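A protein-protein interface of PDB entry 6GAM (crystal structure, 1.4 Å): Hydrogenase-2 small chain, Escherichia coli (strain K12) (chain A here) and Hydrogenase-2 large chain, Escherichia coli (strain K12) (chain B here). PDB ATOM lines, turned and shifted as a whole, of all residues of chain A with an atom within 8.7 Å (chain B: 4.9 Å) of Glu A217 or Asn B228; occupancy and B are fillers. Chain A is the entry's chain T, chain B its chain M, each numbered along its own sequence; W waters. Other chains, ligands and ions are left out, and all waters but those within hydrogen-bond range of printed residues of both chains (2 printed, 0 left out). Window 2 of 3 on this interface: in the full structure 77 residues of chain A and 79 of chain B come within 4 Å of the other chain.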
ATOM      1  N   ARG A 197      33.407   5.490   8.887  1.00  0.00           N
ATOM      2  CA  ARG A 197      32.433   4.831   9.732  1.00  0.00           C
ATOM      3  C   ARG A 197      32.775   3.357  10.033  1.00  0.00           C
ATOM      4  O   ARG A 197      32.039   2.684  10.762  1.00  0.00           O
ATOM      5  CB  ARG A 197      31.037   4.940   9.131  1.00  0.00           C
ATOM      6  CG  ARG A 197      30.641   6.401   8.957  1.00  0.00           C
ATOM      7  CD  ARG A 197      29.205   6.650   8.794  1.00  0.00           C
ATOM      8  NE  ARG A 197      28.976   8.096   8.713  1.00  0.00           N
ATOM      9  CZ  ARG A 197      27.803   8.667   8.871  1.00  0.00           C
ATOM     10  NH1 ARG A 197      26.672   7.994   9.064  1.00  0.00           N
ATOM     11  NH2 ARG A 197      27.754  10.002   8.839  1.00  0.00           N
ATOM     12  N   HIS A 200      32.355   2.038  13.542  1.00  0.00           N
ATOM     13  CA  HIS A 200      30.995   1.725  13.922  1.00  0.00           C
ATOM     14  C   HIS A 200      30.568   0.373  13.363  1.00  0.00           C
ATOM     15  O   HIS A 200      29.970  -0.434  14.086  1.00  0.00           O
ATOM     16  CB  HIS A 200      30.050   2.829  13.447  1.00  0.00           C
ATOM     17  CG  HIS A 200      30.446   4.179  13.951  1.00  0.00           C
ATOM     18  ND1 HIS A 200      30.639   4.427  15.296  1.00  0.00           N
ATOM     19  CD2 HIS A 200      30.811   5.313  13.292  1.00  0.00           C
ATOM     20  CE1 HIS A 200      31.062   5.675  15.439  1.00  0.00           C
ATOM     21  NE2 HIS A 200      31.159   6.234  14.245  1.00  0.00           N
ATOM     22  N   ARG A 205      27.672  -0.892  15.658  1.00  0.00           N
ATOM     23  CA  ARG A 205      26.903   0.342  15.796  1.00  0.00           C
ATOM     24  C   ARG A 205      26.339   0.756  14.436  1.00  0.00           C
ATOM     25  O   ARG A 205      27.036   1.363  13.573  1.00  0.00           O
ATOM     26  CB  ARG A 205      27.759   1.456  16.343  1.00  0.00           C
ATOM     27  CG  ARG A 205      28.142   1.260  17.813  1.00  0.00           C
ATOM     28  CD  ARG A 205      28.858   2.447  18.402  1.00  0.00           C
ATOM     29  NE  ARG A 205      30.100   2.816  17.721  1.00  0.00           N
ATOM     30  CZ  ARG A 205      31.345   2.585  18.146  1.00  0.00           C
ATOM     31  NH1 ARG A 205      31.573   1.913  19.283  1.00  0.00           N
ATOM     32  NH2 ARG A 205      32.380   3.052  17.452  1.00  0.00           N
ATOM     33  N   ALA A 207      23.020   2.371  12.094  1.00  0.00           N
ATOM     34  CA  ALA A 207      21.706   3.011  11.891  1.00  0.00           C
ATOM     35  C   ALA A 207      20.724   1.975  11.395  1.00  0.00           C
ATOM     36  O   ALA A 207      21.091   1.122  10.595  1.00  0.00           O
ATOM     37  CB  ALA A 207      21.831   4.130  10.855  1.00  0.00           C
ATOM     38  N   GLY A 211      16.962   8.887  10.692  1.00  0.00           N
ATOM     39  CA  GLY A 211      16.364   9.679  11.756  1.00  0.00           C
ATOM     40  C   GLY A 211      16.414   8.998  13.121  1.00  0.00           C
ATOM     41  O   GLY A 211      16.006   9.591  14.110  1.00  0.00           O
ATOM     42  N   ASP A 212      16.856   7.744  13.161  1.00  0.00           N
ATOM     43  CA  ASP A 212      16.910   7.050  14.457  1.00  0.00           C
ATOM     44  C   ASP A 212      18.119   7.485  15.233  1.00  0.00           C
ATOM     45  O   ASP A 212      18.930   8.297  14.780  1.00  0.00           O
ATOM     46  CB  ASP A 212      16.774   5.527  14.300  1.00  0.00           C
ATOM     47  CG  ASP A 212      18.044   4.795  13.916  1.00  0.00           C
ATOM     48  OD1 ASP A 212      19.144   5.358  13.757  1.00  0.00           O
ATOM     49  OD2 ASP A 212      17.937   3.543  13.699  1.00  0.00           O
ATOM     50  N   GLU A 213      18.226   6.993  16.455  1.00  0.00           N
ATOM     51  CA  GLU A 213      19.224   7.552  17.360  1.00  0.00           C
ATOM     52  C   GLU A 213      20.636   7.297  16.850  1.00  0.00           C
ATOM     53  O   GLU A 213      21.462   8.231  16.856  1.00  0.00           O
ATOM     54  CB  GLU A 213      19.007   6.955  18.757  1.00  0.00           C
ATOM     55  CG  GLU A 213      19.875   7.556  19.851  1.00  0.00           C
ATOM     56  CD  GLU A 213      19.545   6.908  21.211  1.00  0.00           C
ATOM     57  OE1 GLU A 213      20.322   6.034  21.673  1.00  0.00           O
ATOM     58  OE2 GLU A 213      18.485   7.250  21.775  1.00  0.00           O
ATOM     59  N   GLY A 214      20.925   6.107  16.371  1.00  0.00           N
ATOM     60  CA  GLY A 214      22.214   5.761  15.796  1.00  0.00           C
ATOM     61  C   GLY A 214      22.559   6.586  14.552  1.00  0.00           C
ATOM     62  O   GLY A 214      23.698   7.059  14.360  1.00  0.00           O
ATOM     63  N   HIS A 215      21.565   6.719  13.687  1.00  0.00           N
ATOM     64  CA  HIS A 215      21.750   7.526  12.478  1.00  0.00           C
ATOM     65  C   HIS A 215      22.129   8.966  12.837  1.00  0.00           C
ATOM     66  O   HIS A 215      23.017   9.570  12.204  1.00  0.00           O
ATOM     67  CB  HIS A 215      20.435   7.507  11.713  1.00  0.00           C
ATOM     68  CG  HIS A 215      20.496   8.169  10.368  1.00  0.00           C
ATOM     69  ND1 HIS A 215      19.677   9.219  10.039  1.00  0.00           N
ATOM     70  CD2 HIS A 215      21.293   7.950   9.306  1.00  0.00           C
ATOM     71  CE1 HIS A 215      19.957   9.598   8.800  1.00  0.00           C
ATOM     72  NE2 HIS A 215      20.911   8.834   8.330  1.00  0.00           N
ATOM     73  N   ARG A 216      21.500   9.496  13.879  1.00  0.00           N
ATOM     74  CA  ARG A 216      21.746  10.849  14.401  1.00  0.00           C
ATOM     75  C   ARG A 216      23.017  10.976  15.191  1.00  0.00           C
ATOM     76  O   ARG A 216      23.369  12.068  15.620  1.00  0.00           O
ATOM     77  CB  ARG A 216      20.532  11.392  15.146  1.00  0.00           C
ATOM     78  CG  ARG A 216      19.360  11.617  14.204  1.00  0.00           C
ATOM     79  CD  ARG A 216      18.082  12.054  14.896  1.00  0.00           C
ATOM     80  NE  ARG A 216      18.325  13.296  15.526  1.00  0.00           N
ATOM     81  CZ  ARG A 216      18.307  13.538  16.833  1.00  0.00           C
ATOM     82  NH1 ARG A 216      17.905  12.568  17.701  1.00  0.00           N
ATOM     83  NH2 ARG A 216      18.666  14.776  17.251  1.00  0.00           N
ATOM     84  N   GLU A 217      23.724   9.858  15.326  1.00  0.00           N
ATOM     85  CA  GLU A 217      25.078   9.864  15.866  1.00  0.00           C
ATOM     86  C   GLU A 217      26.140   9.525  14.848  1.00  0.00           C
ATOM     87  O   GLU A 217      27.311   9.329  15.170  1.00  0.00           O
ATOM     88  CB  GLU A 217      25.178   8.921  17.071  1.00  0.00           C
ATOM     89  CG  GLU A 217      24.308   9.319  18.281  1.00  0.00           C
ATOM     90  CD  GLU A 217      24.570  10.736  18.852  1.00  0.00           C
ATOM     91  OE1 GLU A 217      25.704  11.354  18.708  1.00  0.00           O
ATOM     92  OE2 GLU A 217      23.583  11.282  19.424  1.00  0.00           O
ATOM     93  N   GLY A 218      25.767   9.435  13.569  1.00  0.00           N
ATOM     94  CA  GLY A 218      26.760   9.181  12.538  1.00  0.00           C
ATOM     95  C   GLY A 218      27.280   7.767  12.456  1.00  0.00           C
ATOM     96  O   GLY A 218      28.368   7.514  12.040  1.00  0.00           O
ATOM     97  N   TRP A 219      26.452   6.792  12.845  1.00  0.00           N
ATOM     98  CA  TRP A 219      26.860   5.383  12.794  1.00  0.00           C
ATOM     99  C   TRP A 219      26.870   4.787  11.382  1.00  0.00           C
ATOM    100  O   TRP A 219      26.489   5.417  10.399  1.00  0.00           O
ATOM    101  CB  TRP A 219      25.930   4.569  13.728  1.00  0.00           C
ATOM    102  CG  TRP A 219      26.153   4.784  15.185  1.00  0.00           C
ATOM    103  CD1 TRP A 219      27.031   5.602  15.775  1.00  0.00           C
ATOM    104  CD2 TRP A 219      25.433   4.131  16.230  1.00  0.00           C
ATOM    105  NE1 TRP A 219      26.944   5.497  17.174  1.00  0.00           N
ATOM    106  CE2 TRP A 219      25.957   4.593  17.454  1.00  0.00           C
ATOM    107  CE3 TRP A 219      24.430   3.179  16.244  1.00  0.00           C
ATOM    108  CZ2 TRP A 219      25.493   4.127  18.692  1.00  0.00           C
ATOM    109  CZ3 TRP A 219      23.954   2.718  17.499  1.00  0.00           C
ATOM    110  CH2 TRP A 219      24.503   3.187  18.675  1.00  0.00           C
ATOM    111  N   CYS A 220      27.350   3.554  11.266  1.00  0.00           N
ATOM    112  CA  CYS A 220      27.529   2.914  10.002  1.00  0.00           C
ATOM    113  C   CYS A 220      26.199   2.632   9.336  1.00  0.00           C
ATOM    114  O   CYS A 220      25.201   2.402  10.016  1.00  0.00           O
ATOM    115  CB  CYS A 220      28.374   1.629  10.161  1.00  0.00           C
ATOM    116  SG  CYS A 220      28.363   0.469   8.766  1.00  0.00           S
ATOM    117  N   LEU A 221      26.193   2.780   7.999  1.00  0.00           N
ATOM    118  CA  LEU A 221      24.996   2.667   7.175  1.00  0.00           C
ATOM    119  C   LEU A 221      24.830   1.297   6.493  1.00  0.00           C
ATOM    120  O   LEU A 221      23.971   1.130   5.619  1.00  0.00           O
ATOM    121  CB  LEU A 221      24.946   3.809   6.154  1.00  0.00           C
ATOM    122  CG  LEU A 221      25.123   5.209   6.766  1.00  0.00           C
ATOM    123  CD1 LEU A 221      24.960   6.287   5.692  1.00  0.00           C
ATOM    124  CD2 LEU A 221      24.160   5.485   7.915  1.00  0.00           C
ATOM    125  N   PRO B 226      20.633  13.584   9.044  1.00  0.00           N
ATOM    126  CA  PRO B 226      20.283  13.368  10.454  1.00  0.00           C
ATOM    127  C   PRO B 226      20.463  14.703  11.181  1.00  0.00           C
ATOM    128  O   PRO B 226      21.590  15.166  11.327  1.00  0.00           O
ATOM    129  CB  PRO B 226      21.311  12.323  10.912  1.00  0.00           C
ATOM    130  CG  PRO B 226      22.308  12.151   9.799  1.00  0.00           C
ATOM    131  CD  PRO B 226      22.039  13.281   8.816  1.00  0.00           C
ATOM    132  N   ILE B 227      19.373  15.297  11.641  1.00  0.00           N
ATOM    133  CA  ILE B 227      19.429  16.584  12.322  1.00  0.00           C
ATOM    134  C   ILE B 227      19.808  16.362  13.775  1.00  0.00           C
ATOM    135  O   ILE B 227      19.068  15.700  14.527  1.00  0.00           O
ATOM    136  CB  ILE B 227      18.104  17.339  12.256  1.00  0.00           C
ATOM    137  CG1 ILE B 227      17.844  17.743  10.792  1.00  0.00           C
ATOM    138  CG2 ILE B 227      18.128  18.540  13.203  1.00  0.00           C
ATOM    139  CD1 ILE B 227      16.540  18.444  10.529  1.00  0.00           C
ATOM    140  N   ASN B 228      20.937  16.923  14.224  1.00  0.00           N
ATOM    141  CA  ASN B 228      21.340  16.836  15.631  1.00  0.00           C
ATOM    142  C   ASN B 228      22.354  17.950  15.839  1.00  0.00           C
ATOM    143  O   ASN B 228      23.511  17.783  15.495  1.00  0.00           O
ATOM    144  CB  ASN B 228      21.945  15.461  15.969  1.00  0.00           C
ATOM    145  CG  ASN B 228      22.319  15.304  17.413  1.00  0.00           C
ATOM    146  OD1 ASN B 228      22.202  16.242  18.198  1.00  0.00           O
ATOM    147  ND2 ASN B 228      22.814  14.105  17.767  1.00  0.00           N
ATOM    148  N   LEU B 229      21.917  19.039  16.418  1.00  0.00           N
ATOM    149  CA  LEU B 229      22.830  20.178  16.623  1.00  0.00           C
ATOM    150  C   LEU B 229      24.033  19.824  17.426  1.00  0.00           C
ATOM    151  O   LEU B 229      25.078  20.479  17.286  1.00  0.00           O
ATOM    152  CB  LEU B 229      22.126  21.337  17.272  1.00  0.00           C
ATOM    153  CG  LEU B 229      20.990  21.978  16.481  1.00  0.00           C
ATOM    154  CD1 LEU B 229      20.583  23.245  17.195  1.00  0.00           C
ATOM    155  CD2 LEU B 229      21.344  22.312  15.027  1.00  0.00           C
ATOM    156  N   ASP B 230      23.925  18.820  18.292  1.00  0.00           N
ATOM    157  CA  ASP B 230      25.005  18.394  19.191  1.00  0.00           C
ATOM    158  C   ASP B 230      25.748  17.161  18.751  1.00  0.00           C
ATOM    159  O   ASP B 230      26.537  16.640  19.486  1.00  0.00           O
ATOM    160  CB  ASP B 230      24.404  18.246  20.599  1.00  0.00           C
ATOM    161  CG  ASP B 230      23.890  19.562  21.101  1.00  0.00           C
ATOM    162  OD1 ASP B 230      24.697  20.483  21.218  1.00  0.00           O
ATOM    163  OD2 ASP B 230      22.663  19.691  21.329  1.00  0.00           O
ATOM    164  N   GLY B 231      25.493  16.696  17.511  1.00  0.00           N
ATOM    165  CA  GLY B 231      26.081  15.480  17.019  1.00  0.00           C
ATOM    166  C   GLY B 231      27.315  15.655  16.158  1.00  0.00           C
ATOM    167  O   GLY B 231      27.355  16.512  15.285  1.00  0.00           O
ATOM    168  N   LEU B 232      28.309  14.823  16.363  1.00  0.00           N
ATOM    169  CA  LEU B 232      29.489  14.749  15.516  1.00  0.00           C
ATOM    170  C   LEU B 232      29.150  13.972  14.265  1.00  0.00           C
ATOM    171  O   LEU B 232      28.494  12.906  14.335  1.00  0.00           O
ATOM    172  CB  LEU B 232      30.598  14.104  16.334  1.00  0.00           C
ATOM    173  CG  LEU B 232      31.996  14.062  15.740  1.00  0.00           C
ATOM    174  CD1 LEU B 232      33.038  14.132  16.835  1.00  0.00           C
ATOM    175  CD2 LEU B 232      32.188  12.813  14.939  1.00  0.00           C
ATOM    176  N   VAL B 234      27.121  14.613  11.749  1.00  0.00           N
ATOM    177  CA  VAL B 234      25.752  14.730  11.243  1.00  0.00           C
ATOM    178  C   VAL B 234      25.402  16.197  10.966  1.00  0.00           C
ATOM    179  O   VAL B 234      26.304  17.044  10.985  1.00  0.00           O
ATOM    180  CB  VAL B 234      24.779  14.042  12.244  1.00  0.00           C
ATOM    181  CG1 VAL B 234      25.119  12.562  12.417  1.00  0.00           C
ATOM    182  CG2 VAL B 234      24.765  14.730  13.591  1.00  0.00           C
ATOM    183  N   LEU B 235      24.136  16.490  10.666  1.00  0.00           N
ATOM    184  CA  LEU B 235      23.705  17.848  10.320  1.00  0.00           C
ATOM    185  C   LEU B 235      23.544  18.614  11.625  1.00  0.00           C
ATOM    186  O   LEU B 235      22.495  18.604  12.258  1.00  0.00           O
ATOM    187  CB  LEU B 235      22.446  17.823   9.466  1.00  0.00           C
ATOM    188  CG  LEU B 235      21.959  19.180   8.977  1.00  0.00           C
ATOM    189  CD1 LEU B 235      23.054  19.806   8.135  1.00  0.00           C
ATOM    190  CD2 LEU B 235      20.716  19.019   8.146  1.00  0.00           C
ATOM    191  N   ASN B 236      24.636  19.275  11.995  1.00  0.00           N
ATOM    192  CA  ASN B 236      24.723  20.023  13.248  1.00  0.00           C
ATOM    193  C   ASN B 236      24.749  21.514  12.991  1.00  0.00           C
ATOM    194  O   ASN B 236      24.585  21.941  11.849  1.00  0.00           O
ATOM    195  CB  ASN B 236      25.891  19.510  14.069  1.00  0.00           C
ATOM    196  CG  ASN B 236      27.224  19.703  13.391  1.00  0.00           C
ATOM    197  OD1 ASN B 236      27.374  20.633  12.608  1.00  0.00           O
ATOM    198  ND2 ASN B 236      28.220  18.868  13.724  1.00  0.00           N
HETATM  199  O   HOH W   1      27.840  11.889  17.104  1.00  0.00           O
HETATM  200  O   HOH W   2      23.696  13.477  20.624  1.00  0.00           O
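The guanidinium group (NE) of Arg A216 is in hydrogen-bond range of the backbone carbonyl oxygen (O) of Ile B227 (2.7 Å). The backbone carbonyl oxygen (O) of Arg A216 lies within hydrogen-bond range of the side-chain amide nitrogen (ND2) of Asn B228 (3.0 Å). The side-chain amide nitrogen (ND2) of Asn B228 sits at hydrogen-bond distance from the side-chain carboxylate (OE2) of Glu A217.
The backbone carbonyl oxygen (O) of Gly A218 sits close to the guanidinium group (NE) of Arg A197 (3.4 Å). The backbone NH (N) of Gly A211 sits at hydrogen-bond distance from a ring nitrogen (ND1) of His A215 (2.8 Å). O of Pro B226 sits at hydrogen-bond distance from N of Leu B235. The backbone NH of Asp B230 sits close to the side-chain amide oxygen of Asn B228 (3.1 Å). The backbone NH (N) of Gly B231 sits at hydrogen-bond distance from the side-chain amide oxygen (OD1) of Asn B228 (3.4 Å). The backbone NH (N) of Asn B228 sits at hydrogen-bond distance from the backbone carbonyl oxygen (O) of Leu B235.
Pro B226 touches His A215. Val B234 touches His A215. CB of Pro B226 touches CA of Arg A216, 3.8 Å away. O of Arg A216 touches CG2 of Val B234, at 3.6 Å. Leu B232 touches Glu A217. N of Gly A218 touches CG1 of Val B234 (3.4 Å).
Arg A205 touches none of the printed residues of chain B. Glu A217 touches just these residues of chain B: Asn B228 (3.4 Å) and Leu B232 (3.9 Å). Of chain A, only Arg A216 (3.0 Å) and Glu A217 (3.4 Å) come within 4 Å of Asn B228. No residue of chain A comes within 4 Å of Gly B231. Of the printed residues of chain A, Leu B232 touches Glu A217 (3.9 Å). Of the printed residues of chain A, Val B234 touches His A215, Arg A216 and Gly A218. The nearest residue of chain A that does not touch Asn B228 is Glu A213 (6.1 Å). The nearest printed residue of chain A that does not touch Leu B232 is Gly A218 (4.5 Å).
Hydrophobic or aromatic side chains of chain B that line the printed part of chain A: Pro B226 and Val B234. Of the 15 printed residues of chain A, 4 touch a printed residue of chain B. Printed residues of chain A that touch a printed residue of chain B: His A215, Arg A216, Glu A217 and Gly A218. Among the printed residues, 9 pairs touch across the chains. Among the printed residues, no Asp or Glu carboxylate lies within 4 Å of a Lys or Arg side-chain nitrogen of the other chain.
Water W2 lies within hydrogen-bond range of the side-chain carboxylate of Glu A217 and the side-chain amide nitrogen of Asn B228. Water W1 lies within hydrogen-bond range of the side-chain carboxylate of Glu A217 (2.7 Å) and the backbone carbonyl oxygen of Leu B232 (3.0 Å).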
